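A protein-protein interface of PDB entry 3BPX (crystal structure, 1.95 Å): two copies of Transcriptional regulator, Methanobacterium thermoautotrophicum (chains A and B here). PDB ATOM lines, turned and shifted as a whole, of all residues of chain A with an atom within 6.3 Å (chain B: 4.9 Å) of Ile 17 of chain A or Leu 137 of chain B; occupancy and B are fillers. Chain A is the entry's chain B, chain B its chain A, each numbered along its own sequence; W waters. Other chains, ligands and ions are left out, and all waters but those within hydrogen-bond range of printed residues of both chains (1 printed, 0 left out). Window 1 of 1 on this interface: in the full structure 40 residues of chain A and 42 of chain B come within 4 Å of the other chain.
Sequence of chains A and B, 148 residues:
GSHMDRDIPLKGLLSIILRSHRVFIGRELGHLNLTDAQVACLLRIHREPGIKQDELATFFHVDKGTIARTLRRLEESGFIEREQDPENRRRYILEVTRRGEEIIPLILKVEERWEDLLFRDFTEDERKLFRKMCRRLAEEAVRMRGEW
No position is printed for both chains.
The backbone carbonyl oxygen of Ile 17 of chain A is in hydrogen-bond range of the side-chain hydroxyl of Ser 20 of chain A (2.6 Å). OG of Ser 20 of chain A is in hydrogen-bond range of NE1 of Trp 114 of chain A (3.1 Å).
Of the 9 printed residues of chain B, 7 touch a printed residue of chain A. Of the 16 printed residues of chain A, 9 touch a printed residue of chain B. Printed residues of chain A that touch a printed residue of chain B: Leu 13, Leu 14, Ile 16, Ile 17, Ser 20, Leu 118, Phe 119, Phe 122 and Phe 130.
Water W1 lies within hydrogen-bond range of the backbone carbonyl oxygen of Leu 118 of chain A and the side-chain carboxylate of Glu 140 of chain B.
Among the printed residues, pairs that only touch across the chains: Leu 118 of chain A with Glu 140 of chain B, Phe 130 of chain A with Leu 137 of chain B, Leu 118 of chain A with Leu 137 of chain B, Phe 122 of chain A with Leu 137 of chain B, Phe 130 of chain A with Met 133 of chain B, Ser 20 of chain A with Ala 141 of chain B, Phe 122 of chain A with Arg 136 of chain B, Ile 17 of chain A with Leu 137 of chain B, Ile 16 of chain A with Ala 138 of chain B, Phe 122 of chain A with Met 133 of chain B, Phe 130 of chain A with Cys 134 of chain B, Ile 17 of chain A with Cys 134 of chain B, Ile 17 of chain A with Ala 138 of chain B, Leu 14 of chain A with Cys 134 of chain B, Ile 16 of chain A with Ala 141 of chain B, Phe 119 of chain A with Leu 137 of chain B and Leu 13 of chain A with Ala 138 of chain B.
Gly 12 of chain A touches none of the printed residues of chain B. Ile 17 of chain A touches just these residues of chain B: Cys 134 (3.7 Å), Leu 137 (3.7 Å) and Ala 138 (3.7 Å). Printed residues of chain A within 4 Å of Cys 134 of chain B: Leu 14, Ile 17 and Phe 130. Printed residues of chain A within 4 Å of Arg 136 of chain B: Phe 122. Of chain A, only Ile 17, Leu 118, Phe 119, Phe 122 and Phe 130 come within 4 Å of Leu 137 of chain B. Of the printed residues of chain A, Ala 141 of chain B touches Ile 16 (3.9 Å) and Ser 20 (3.6 Å). The nearest residue of chain A that does not touch Leu 137 of chain B is Ile 16 of chain A (5.7 Å). The nearest printed residue of chain A that does not touch Arg 136 of chain B is Leu 118 of chain A (5.7 Å).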
ATOM      1  N   GLY A  12       2.966 -13.600 -15.423  1.00  0.00           N
ATOM      2  CA  GLY A  12       3.853 -13.024 -14.431  1.00  0.00           C
ATOM      3  C   GLY A  12       5.262 -12.915 -14.965  1.00  0.00           C
ATOM      4  O   GLY A  12       5.941 -11.920 -14.738  1.00  0.00           O
ATOM      5  N   LEU A  13       5.705 -13.945 -15.684  1.00  0.00           N
ATOM      6  CA  LEU A  13       7.043 -13.949 -16.259  1.00  0.00           C
ATOM      7  C   LEU A  13       7.184 -12.890 -17.350  1.00  0.00           C
ATOM      8  O   LEU A  13       8.205 -12.216 -17.444  1.00  0.00           O
ATOM      9  CB  LEU A  13       7.362 -15.335 -16.835  1.00  0.00           C
ATOM     10  CG  LEU A  13       7.299 -16.465 -15.803  1.00  0.00           C
ATOM     11  CD1 LEU A  13       7.462 -17.830 -16.481  1.00  0.00           C
ATOM     12  CD2 LEU A  13       8.380 -16.243 -14.769  1.00  0.00           C
ATOM     13  N   LEU A  14       6.154 -12.746 -18.176  1.00  0.00           N
ATOM     14  CA  LEU A  14       6.189 -11.759 -19.250  1.00  0.00           C
ATOM     15  C   LEU A  14       6.127 -10.343 -18.690  1.00  0.00           C
ATOM     16  O   LEU A  14       6.760  -9.432 -19.215  1.00  0.00           O
ATOM     17  CB  LEU A  14       5.030 -11.998 -20.218  1.00  0.00           C
ATOM     18  CG  LEU A  14       4.979 -13.413 -20.821  1.00  0.00           C
ATOM     19  CD1 LEU A  14       3.604 -13.662 -21.426  1.00  0.00           C
ATOM     20  CD2 LEU A  14       6.081 -13.583 -21.873  1.00  0.00           C
ATOM     21  N   SER A  15       5.365 -10.158 -17.618  1.00  0.00           N
ATOM     22  CA  SER A  15       5.244  -8.845 -16.994  1.00  0.00           C
ATOM     23  C   SER A  15       6.601  -8.425 -16.447  1.00  0.00           C
ATOM     24  O   SER A  15       7.031  -7.288 -16.628  1.00  0.00           O
ATOM     25  CB  SER A  15       4.220  -8.887 -15.854  1.00  0.00           C
ATOM     26  OG  SER A  15       2.934  -9.226 -16.337  1.00  0.00           O
ATOM     27  N   ILE A  16       7.265  -9.356 -15.770  1.00  0.00           N
ATOM     28  CA  ILE A  16       8.588  -9.106 -15.192  1.00  0.00           C
ATOM     29  C   ILE A  16       9.549  -8.645 -16.289  1.00  0.00           C
ATOM     30  O   ILE A  16      10.234  -7.635 -16.149  1.00  0.00           O
ATOM     31  CB  ILE A  16       9.116 -10.397 -14.515  1.00  0.00           C
ATOM     32  CG1 ILE A  16       8.344 -10.633 -13.212  1.00  0.00           C
ATOM     33  CG2 ILE A  16      10.608 -10.311 -14.267  1.00  0.00           C
ATOM     34  CD1 ILE A  16       8.582 -11.990 -12.569  1.00  0.00           C
ATOM     35  N   ILE A  17       9.587  -9.387 -17.387  1.00  0.00           N
ATOM     36  CA  ILE A  17      10.446  -9.052 -18.523  1.00  0.00           C
ATOM     37  C   ILE A  17      10.122  -7.668 -19.107  1.00  0.00           C
ATOM     38  O   ILE A  17      10.991  -6.794 -19.227  1.00  0.00           O
ATOM     39  CB  ILE A  17      10.287 -10.119 -19.623  1.00  0.00           C
ATOM     40  CG1 ILE A  17      10.741 -11.475 -19.075  1.00  0.00           C
ATOM     41  CG2 ILE A  17      11.088  -9.744 -20.859  1.00  0.00           C
ATOM     42  CD1 ILE A  17      10.432 -12.624 -19.980  1.00  0.00           C
ATOM     43  N   LEU A  18       8.863  -7.465 -19.462  1.00  0.00           N
ATOM     44  CA  LEU A  18       8.441  -6.200 -20.035  1.00  0.00           C
ATOM     45  C   LEU A  18       8.701  -5.046 -19.071  1.00  0.00           C
ATOM     46  O   LEU A  18       8.961  -3.922 -19.499  1.00  0.00           O
ATOM     47  CB  LEU A  18       6.955  -6.264 -20.385  1.00  0.00           C
ATOM     48  CG  LEU A  18       6.367  -5.001 -21.017  1.00  0.00           C
ATOM     49  CD1 LEU A  18       7.176  -4.615 -22.259  1.00  0.00           C
ATOM     50  CD2 LEU A  18       4.904  -5.252 -21.375  1.00  0.00           C
ATOM     51  N   ARG A  19       8.634  -5.332 -17.772  1.00  0.00           N
ATOM     52  CA  ARG A  19       8.862  -4.314 -16.747  1.00  0.00           C
ATOM     53  C   ARG A  19      10.283  -3.744 -16.799  1.00  0.00           C
ATOM     54  O   ARG A  19      10.492  -2.564 -16.554  1.00  0.00           O
ATOM     55  CB  ARG A  19       8.588  -4.907 -15.358  1.00  0.00           C
ATOM     56  CG  ARG A  19       8.454  -3.884 -14.250  1.00  0.00           C
ATOM     57  CD  ARG A  19       7.935  -4.544 -12.979  1.00  0.00           C
ATOM     58  NE  ARG A  19       6.638  -5.176 -13.210  1.00  0.00           N
ATOM     59  CZ  ARG A  19       6.293  -6.372 -12.743  1.00  0.00           C
ATOM     60  NH1 ARG A  19       7.150  -7.072 -12.010  1.00  0.00           N
ATOM     61  NH2 ARG A  19       5.098  -6.874 -13.028  1.00  0.00           N
ATOM     62  N   SER A  20      11.258  -4.585 -17.122  1.00  0.00           N
ATOM     63  CA  SER A  20      12.636  -4.117 -17.192  1.00  0.00           C
ATOM     64  C   SER A  20      12.830  -3.200 -18.397  1.00  0.00           C
ATOM     65  O   SER A  20      13.706  -2.339 -18.400  1.00  0.00           O
ATOM     66  CB  SER A  20      13.604  -5.302 -17.271  1.00  0.00           C
ATOM     67  OG  SER A  20      13.397  -6.051 -18.447  1.00  0.00           O
ATOM     68  N   HIS A  21      12.007  -3.387 -19.422  1.00  0.00           N
ATOM     69  CA  HIS A  21      12.095  -2.565 -20.614  1.00  0.00           C
ATOM     70  C   HIS A  21      11.536  -1.195 -20.261  1.00  0.00           C
ATOM     71  O   HIS A  21      12.090  -0.175 -20.652  1.00  0.00           O
ATOM     72  CB  HIS A  21      11.300  -3.173 -21.758  1.00  0.00           C
ATOM     73  CG  HIS A  21      11.201  -2.283 -22.957  1.00  0.00           C
ATOM     74  ND1 HIS A  21      10.359  -1.194 -23.009  1.00  0.00           N
ATOM     75  CD2 HIS A  21      11.853  -2.311 -24.145  1.00  0.00           C
ATOM     76  CE1 HIS A  21      10.495  -0.588 -24.176  1.00  0.00           C
ATOM     77  NE2 HIS A  21      11.394  -1.247 -24.884  1.00  0.00           N
ATOM     78  N   ARG A  22      10.436  -1.191 -19.514  1.00  0.00           N
ATOM     79  CA  ARG A  22       9.787   0.041 -19.083  1.00  0.00           C
ATOM     80  C   ARG A  22      10.758   0.849 -18.221  1.00  0.00           C
ATOM     81  O   ARG A  22      10.871   2.067 -18.361  1.00  0.00           O
ATOM     82  CB  ARG A  22       8.531  -0.295 -18.271  1.00  0.00           C
ATOM     83  CG  ARG A  22       7.574   0.867 -18.035  1.00  0.00           C
ATOM     84  CD  ARG A  22       6.524   0.493 -16.990  1.00  0.00           C
ATOM     85  NE  ARG A  22       6.130  -0.909 -17.106  1.00  0.00           N
ATOM     86  CZ  ARG A  22       5.492  -1.428 -18.151  1.00  0.00           C
ATOM     87  NH1 ARG A  22       5.161  -0.660 -19.180  1.00  0.00           N
ATOM     88  NH2 ARG A  22       5.206  -2.722 -18.177  1.00  0.00           N
ATOM     89  N   TRP A 114      18.379  -2.952 -24.984  1.00  0.00           N
ATOM     90  CA  TRP A 114      17.583  -3.613 -23.966  1.00  0.00           C
ATOM     91  C   TRP A 114      17.506  -5.092 -24.321  1.00  0.00           C
ATOM     92  O   TRP A 114      17.632  -5.956 -23.454  1.00  0.00           O
ATOM     93  CB  TRP A 114      16.163  -3.048 -23.878  1.00  0.00           C
ATOM     94  CG  TRP A 114      15.314  -3.886 -22.945  1.00  0.00           C
ATOM     95  CD1 TRP A 114      15.419  -3.957 -21.584  1.00  0.00           C
ATOM     96  CD2 TRP A 114      14.327  -4.852 -23.320  1.00  0.00           C
ATOM     97  NE1 TRP A 114      14.562  -4.912 -21.089  1.00  0.00           N
ATOM     98  CE2 TRP A 114      13.879  -5.476 -22.134  1.00  0.00           C
ATOM     99  CE3 TRP A 114      13.778  -5.252 -24.543  1.00  0.00           C
ATOM    100  CZ2 TRP A 114      12.909  -6.479 -22.135  1.00  0.00           C
ATOM    101  CZ3 TRP A 114      12.808  -6.255 -24.543  1.00  0.00           C
ATOM    102  CH2 TRP A 114      12.387  -6.853 -23.346  1.00  0.00           C
ATOM    103  N   LEU A 118      18.922  -8.374 -22.155  1.00  0.00           N
ATOM    104  CA  LEU A 118      18.009  -9.459 -21.777  1.00  0.00           C
ATOM    105  C   LEU A 118      18.464 -10.833 -22.275  1.00  0.00           C
ATOM    106  O   LEU A 118      18.279 -11.834 -21.586  1.00  0.00           O
ATOM    107  CB  LEU A 118      16.603  -9.178 -22.328  1.00  0.00           C
ATOM    108  CG  LEU A 118      15.464 -10.088 -21.843  1.00  0.00           C
ATOM    109  CD1 LEU A 118      15.050  -9.683 -20.424  1.00  0.00           C
ATOM    110  CD2 LEU A 118      14.273  -9.991 -22.795  1.00  0.00           C
ATOM    111  N   PHE A 119      19.051 -10.865 -23.470  1.00  0.00           N
ATOM    112  CA  PHE A 119      19.504 -12.109 -24.090  1.00  0.00           C
ATOM    113  C   PHE A 119      20.982 -12.414 -23.881  1.00  0.00           C
ATOM    114  O   PHE A 119      21.537 -13.269 -24.569  1.00  0.00           O
ATOM    115  CB  PHE A 119      19.237 -12.076 -25.599  1.00  0.00           C
ATOM    116  CG  PHE A 119      17.790 -12.182 -25.976  1.00  0.00           C
ATOM    117  CD1 PHE A 119      17.093 -13.369 -25.790  1.00  0.00           C
ATOM    118  CD2 PHE A 119      17.135 -11.107 -26.569  1.00  0.00           C
ATOM    119  CE1 PHE A 119      15.770 -13.490 -26.190  1.00  0.00           C
ATOM    120  CE2 PHE A 119      15.805 -11.217 -26.973  1.00  0.00           C
ATOM    121  CZ  PHE A 119      15.123 -12.411 -26.784  1.00  0.00           C
ATOM    122  N   PHE A 122      21.684 -15.963 -23.671  1.00  0.00           N
ATOM    123  CA  PHE A 122      20.987 -16.728 -24.705  1.00  0.00           C
ATOM    124  C   PHE A 122      21.875 -16.805 -25.936  1.00  0.00           C
ATOM    125  O   PHE A 122      22.539 -15.836 -26.286  1.00  0.00           O
ATOM    126  CB  PHE A 122      19.678 -16.038 -25.104  1.00  0.00           C
ATOM    127  CG  PHE A 122      18.470 -16.528 -24.356  1.00  0.00           C
ATOM    128  CD1 PHE A 122      18.497 -16.680 -22.972  1.00  0.00           C
ATOM    129  CD2 PHE A 122      17.292 -16.809 -25.039  1.00  0.00           C
ATOM    130  CE1 PHE A 122      17.360 -17.106 -22.278  1.00  0.00           C
ATOM    131  CE2 PHE A 122      16.155 -17.231 -24.364  1.00  0.00           C
ATOM    132  CZ  PHE A 122      16.189 -17.381 -22.973  1.00  0.00           C
ATOM    133  N   PHE A 130      13.051 -17.846 -29.551  1.00  0.00           N
ATOM    134  CA  PHE A 130      12.192 -17.170 -28.592  1.00  0.00           C
ATOM    135  C   PHE A 130      11.435 -16.065 -29.313  1.00  0.00           C
ATOM    136  O   PHE A 130      10.229 -15.905 -29.128  1.00  0.00           O
ATOM    137  CB  PHE A 130      12.998 -16.558 -27.448  1.00  0.00           C
ATOM    138  CG  PHE A 130      12.138 -15.956 -26.372  1.00  0.00           C
ATOM    139  CD1 PHE A 130      11.506 -16.766 -25.437  1.00  0.00           C
ATOM    140  CD2 PHE A 130      11.902 -14.581 -26.337  1.00  0.00           C
ATOM    141  CE1 PHE A 130      10.647 -16.220 -24.481  1.00  0.00           C
ATOM    142  CE2 PHE A 130      11.046 -14.025 -25.388  1.00  0.00           C
ATOM    143  CZ  PHE A 130      10.416 -14.848 -24.457  1.00  0.00           C
ATOM    144  N   MET B 133      12.085 -20.767 -21.396  1.00  0.00           N
ATOM    145  CA  MET B 133      12.822 -19.613 -21.886  1.00  0.00           C
ATOM    146  C   MET B 133      12.344 -18.341 -21.187  1.00  0.00           C
ATOM    147  O   MET B 133      13.149 -17.461 -20.860  1.00  0.00           O
ATOM    148  CB  MET B 133      12.668 -19.477 -23.407  1.00  0.00           C
ATOM    149  CG  MET B 133      13.469 -20.504 -24.213  1.00  0.00           C
ATOM    150  SD  MET B 133      13.669 -20.023 -25.948  1.00  0.00           S
ATOM    151  CE  MET B 133      12.094 -20.461 -26.588  1.00  0.00           C
ATOM    152  N   CYS B 134      11.042 -18.243 -20.946  1.00  0.00           N
ATOM    153  CA  CYS B 134      10.512 -17.071 -20.269  1.00  0.00           C
ATOM    154  C   CYS B 134      11.112 -16.927 -18.876  1.00  0.00           C
ATOM    155  O   CYS B 134      11.512 -15.838 -18.474  1.00  0.00           O
ATOM    156  CB  CYS B 134       8.989 -17.147 -20.186  1.00  0.00           C
ATOM    157  SG  CYS B 134       8.201 -16.742 -21.750  1.00  0.00           S
ATOM    158  N   ARG B 135      11.191 -18.032 -18.144  1.00  0.00           N
ATOM    159  CA  ARG B 135      11.759 -18.013 -16.799  1.00  0.00           C
ATOM    160  C   ARG B 135      13.209 -17.518 -16.831  1.00  0.00           C
ATOM    161  O   ARG B 135      13.612 -16.674 -16.031  1.00  0.00           O
ATOM    162  CB  ARG B 135      11.707 -19.414 -16.204  1.00  0.00           C
ATOM    163  CG  ARG B 135      12.245 -19.516 -14.798  1.00  0.00           C
ATOM    164  CD  ARG B 135      12.290 -20.973 -14.360  1.00  0.00           C
ATOM    165  NE  ARG B 135      11.103 -21.715 -14.791  1.00  0.00           N
ATOM    166  CZ  ARG B 135       9.853 -21.401 -14.460  1.00  0.00           C
ATOM    167  NH1 ARG B 135       9.611 -20.351 -13.686  1.00  0.00           N
ATOM    168  NH2 ARG B 135       8.840 -22.136 -14.908  1.00  0.00           N
ATOM    169  N   ARG B 136      13.995 -18.057 -17.757  1.00  0.00           N
ATOM    170  CA  ARG B 136      15.388 -17.660 -17.887  1.00  0.00           C
ATOM    171  C   ARG B 136      15.497 -16.159 -18.144  1.00  0.00           C
ATOM    172  O   ARG B 136      16.360 -15.487 -17.590  1.00  0.00           O
ATOM    173  CB  ARG B 136      16.048 -18.436 -19.032  1.00  0.00           C
ATOM    174  CG  ARG B 136      16.188 -19.936 -18.776  1.00  0.00           C
ATOM    175  CD  ARG B 136      16.638 -20.665 -20.037  1.00  0.00           C
ATOM    176  NE  ARG B 136      17.929 -20.181 -20.520  1.00  0.00           N
ATOM    177  CZ  ARG B 136      18.458 -20.499 -21.699  1.00  0.00           C
ATOM    178  NH1 ARG B 136      17.814 -21.308 -22.527  1.00  0.00           N
ATOM    179  NH2 ARG B 136      19.625 -19.992 -22.060  1.00  0.00           N
ATOM    180  N   LEU B 137      14.600 -15.631 -18.969  1.00  0.00           N
ATOM    181  CA  LEU B 137      14.617 -14.210 -19.305  1.00  0.00           C
ATOM    182  C   LEU B 137      14.099 -13.333 -18.166  1.00  0.00           C
ATOM    183  O   LEU B 137      14.568 -12.204 -17.970  1.00  0.00           O
ATOM    184  CB  LEU B 137      13.806 -13.981 -20.582  1.00  0.00           C
ATOM    185  CG  LEU B 137      14.408 -14.681 -21.806  1.00  0.00           C
ATOM    186  CD1 LEU B 137      13.466 -14.588 -22.994  1.00  0.00           C
ATOM    187  CD2 LEU B 137      15.763 -14.051 -22.121  1.00  0.00           C
ATOM    188  N   ALA B 138      13.128 -13.849 -17.419  1.00  0.00           N
ATOM    189  CA  ALA B 138      12.589 -13.108 -16.290  1.00  0.00           C
ATOM    190  C   ALA B 138      13.715 -13.024 -15.277  1.00  0.00           C
ATOM    191  O   ALA B 138      13.865 -12.028 -14.576  1.00  0.00           O
ATOM    192  CB  ALA B 138      11.405 -13.832 -15.696  1.00  0.00           C
ATOM    193  N   GLU B 139      14.521 -14.075 -15.214  1.00  0.00           N
ATOM    194  CA  GLU B 139      15.633 -14.084 -14.287  1.00  0.00           C
ATOM    195  C   GLU B 139      16.671 -13.048 -14.711  1.00  0.00           C
ATOM    196  O   GLU B 139      17.283 -12.393 -13.868  1.00  0.00           O
ATOM    197  CB  GLU B 139      16.247 -15.488 -14.210  1.00  0.00           C
ATOM    198  CG  GLU B 139      15.367 -16.478 -13.462  1.00  0.00           C
ATOM    199  CD  GLU B 139      15.862 -17.906 -13.542  1.00  0.00           C
ATOM    200  OE1 GLU B 139      15.286 -18.763 -12.836  1.00  0.00           O
ATOM    201  OE2 GLU B 139      16.814 -18.179 -14.309  1.00  0.00           O
ATOM    202  N   GLU B 140      16.845 -12.879 -16.017  1.00  0.00           N
ATOM    203  CA  GLU B 140      17.799 -11.905 -16.527  1.00  0.00           C
ATOM    204  C   GLU B 140      17.320 -10.489 -16.226  1.00  0.00           C
ATOM    205  O   GLU B 140      18.115  -9.634 -15.849  1.00  0.00           O
ATOM    206  CB  GLU B 140      17.988 -12.065 -18.031  1.00  0.00           C
ATOM    207  CG  GLU B 140      19.042 -11.131 -18.605  1.00  0.00           C
ATOM    208  CD  GLU B 140      20.432 -11.451 -18.089  1.00  0.00           C
ATOM    209  OE1 GLU B 140      20.923 -12.564 -18.387  1.00  0.00           O
ATOM    210  OE2 GLU B 140      21.026 -10.594 -17.390  1.00  0.00           O
ATOM    211  N   ALA B 141      16.021 -10.251 -16.398  1.00  0.00           N
ATOM    212  CA  ALA B 141      15.441  -8.940 -16.127  1.00  0.00           C
ATOM    213  C   ALA B 141      15.686  -8.569 -14.666  1.00  0.00           C
ATOM    214  O   ALA B 141      15.979  -7.417 -14.350  1.00  0.00           O
ATOM    215  CB  ALA B 141      13.932  -8.950 -16.412  1.00  0.00           C
HETATM  216  O   HOH W   1      19.940 -13.876 -21.031  1.00  0.00           O
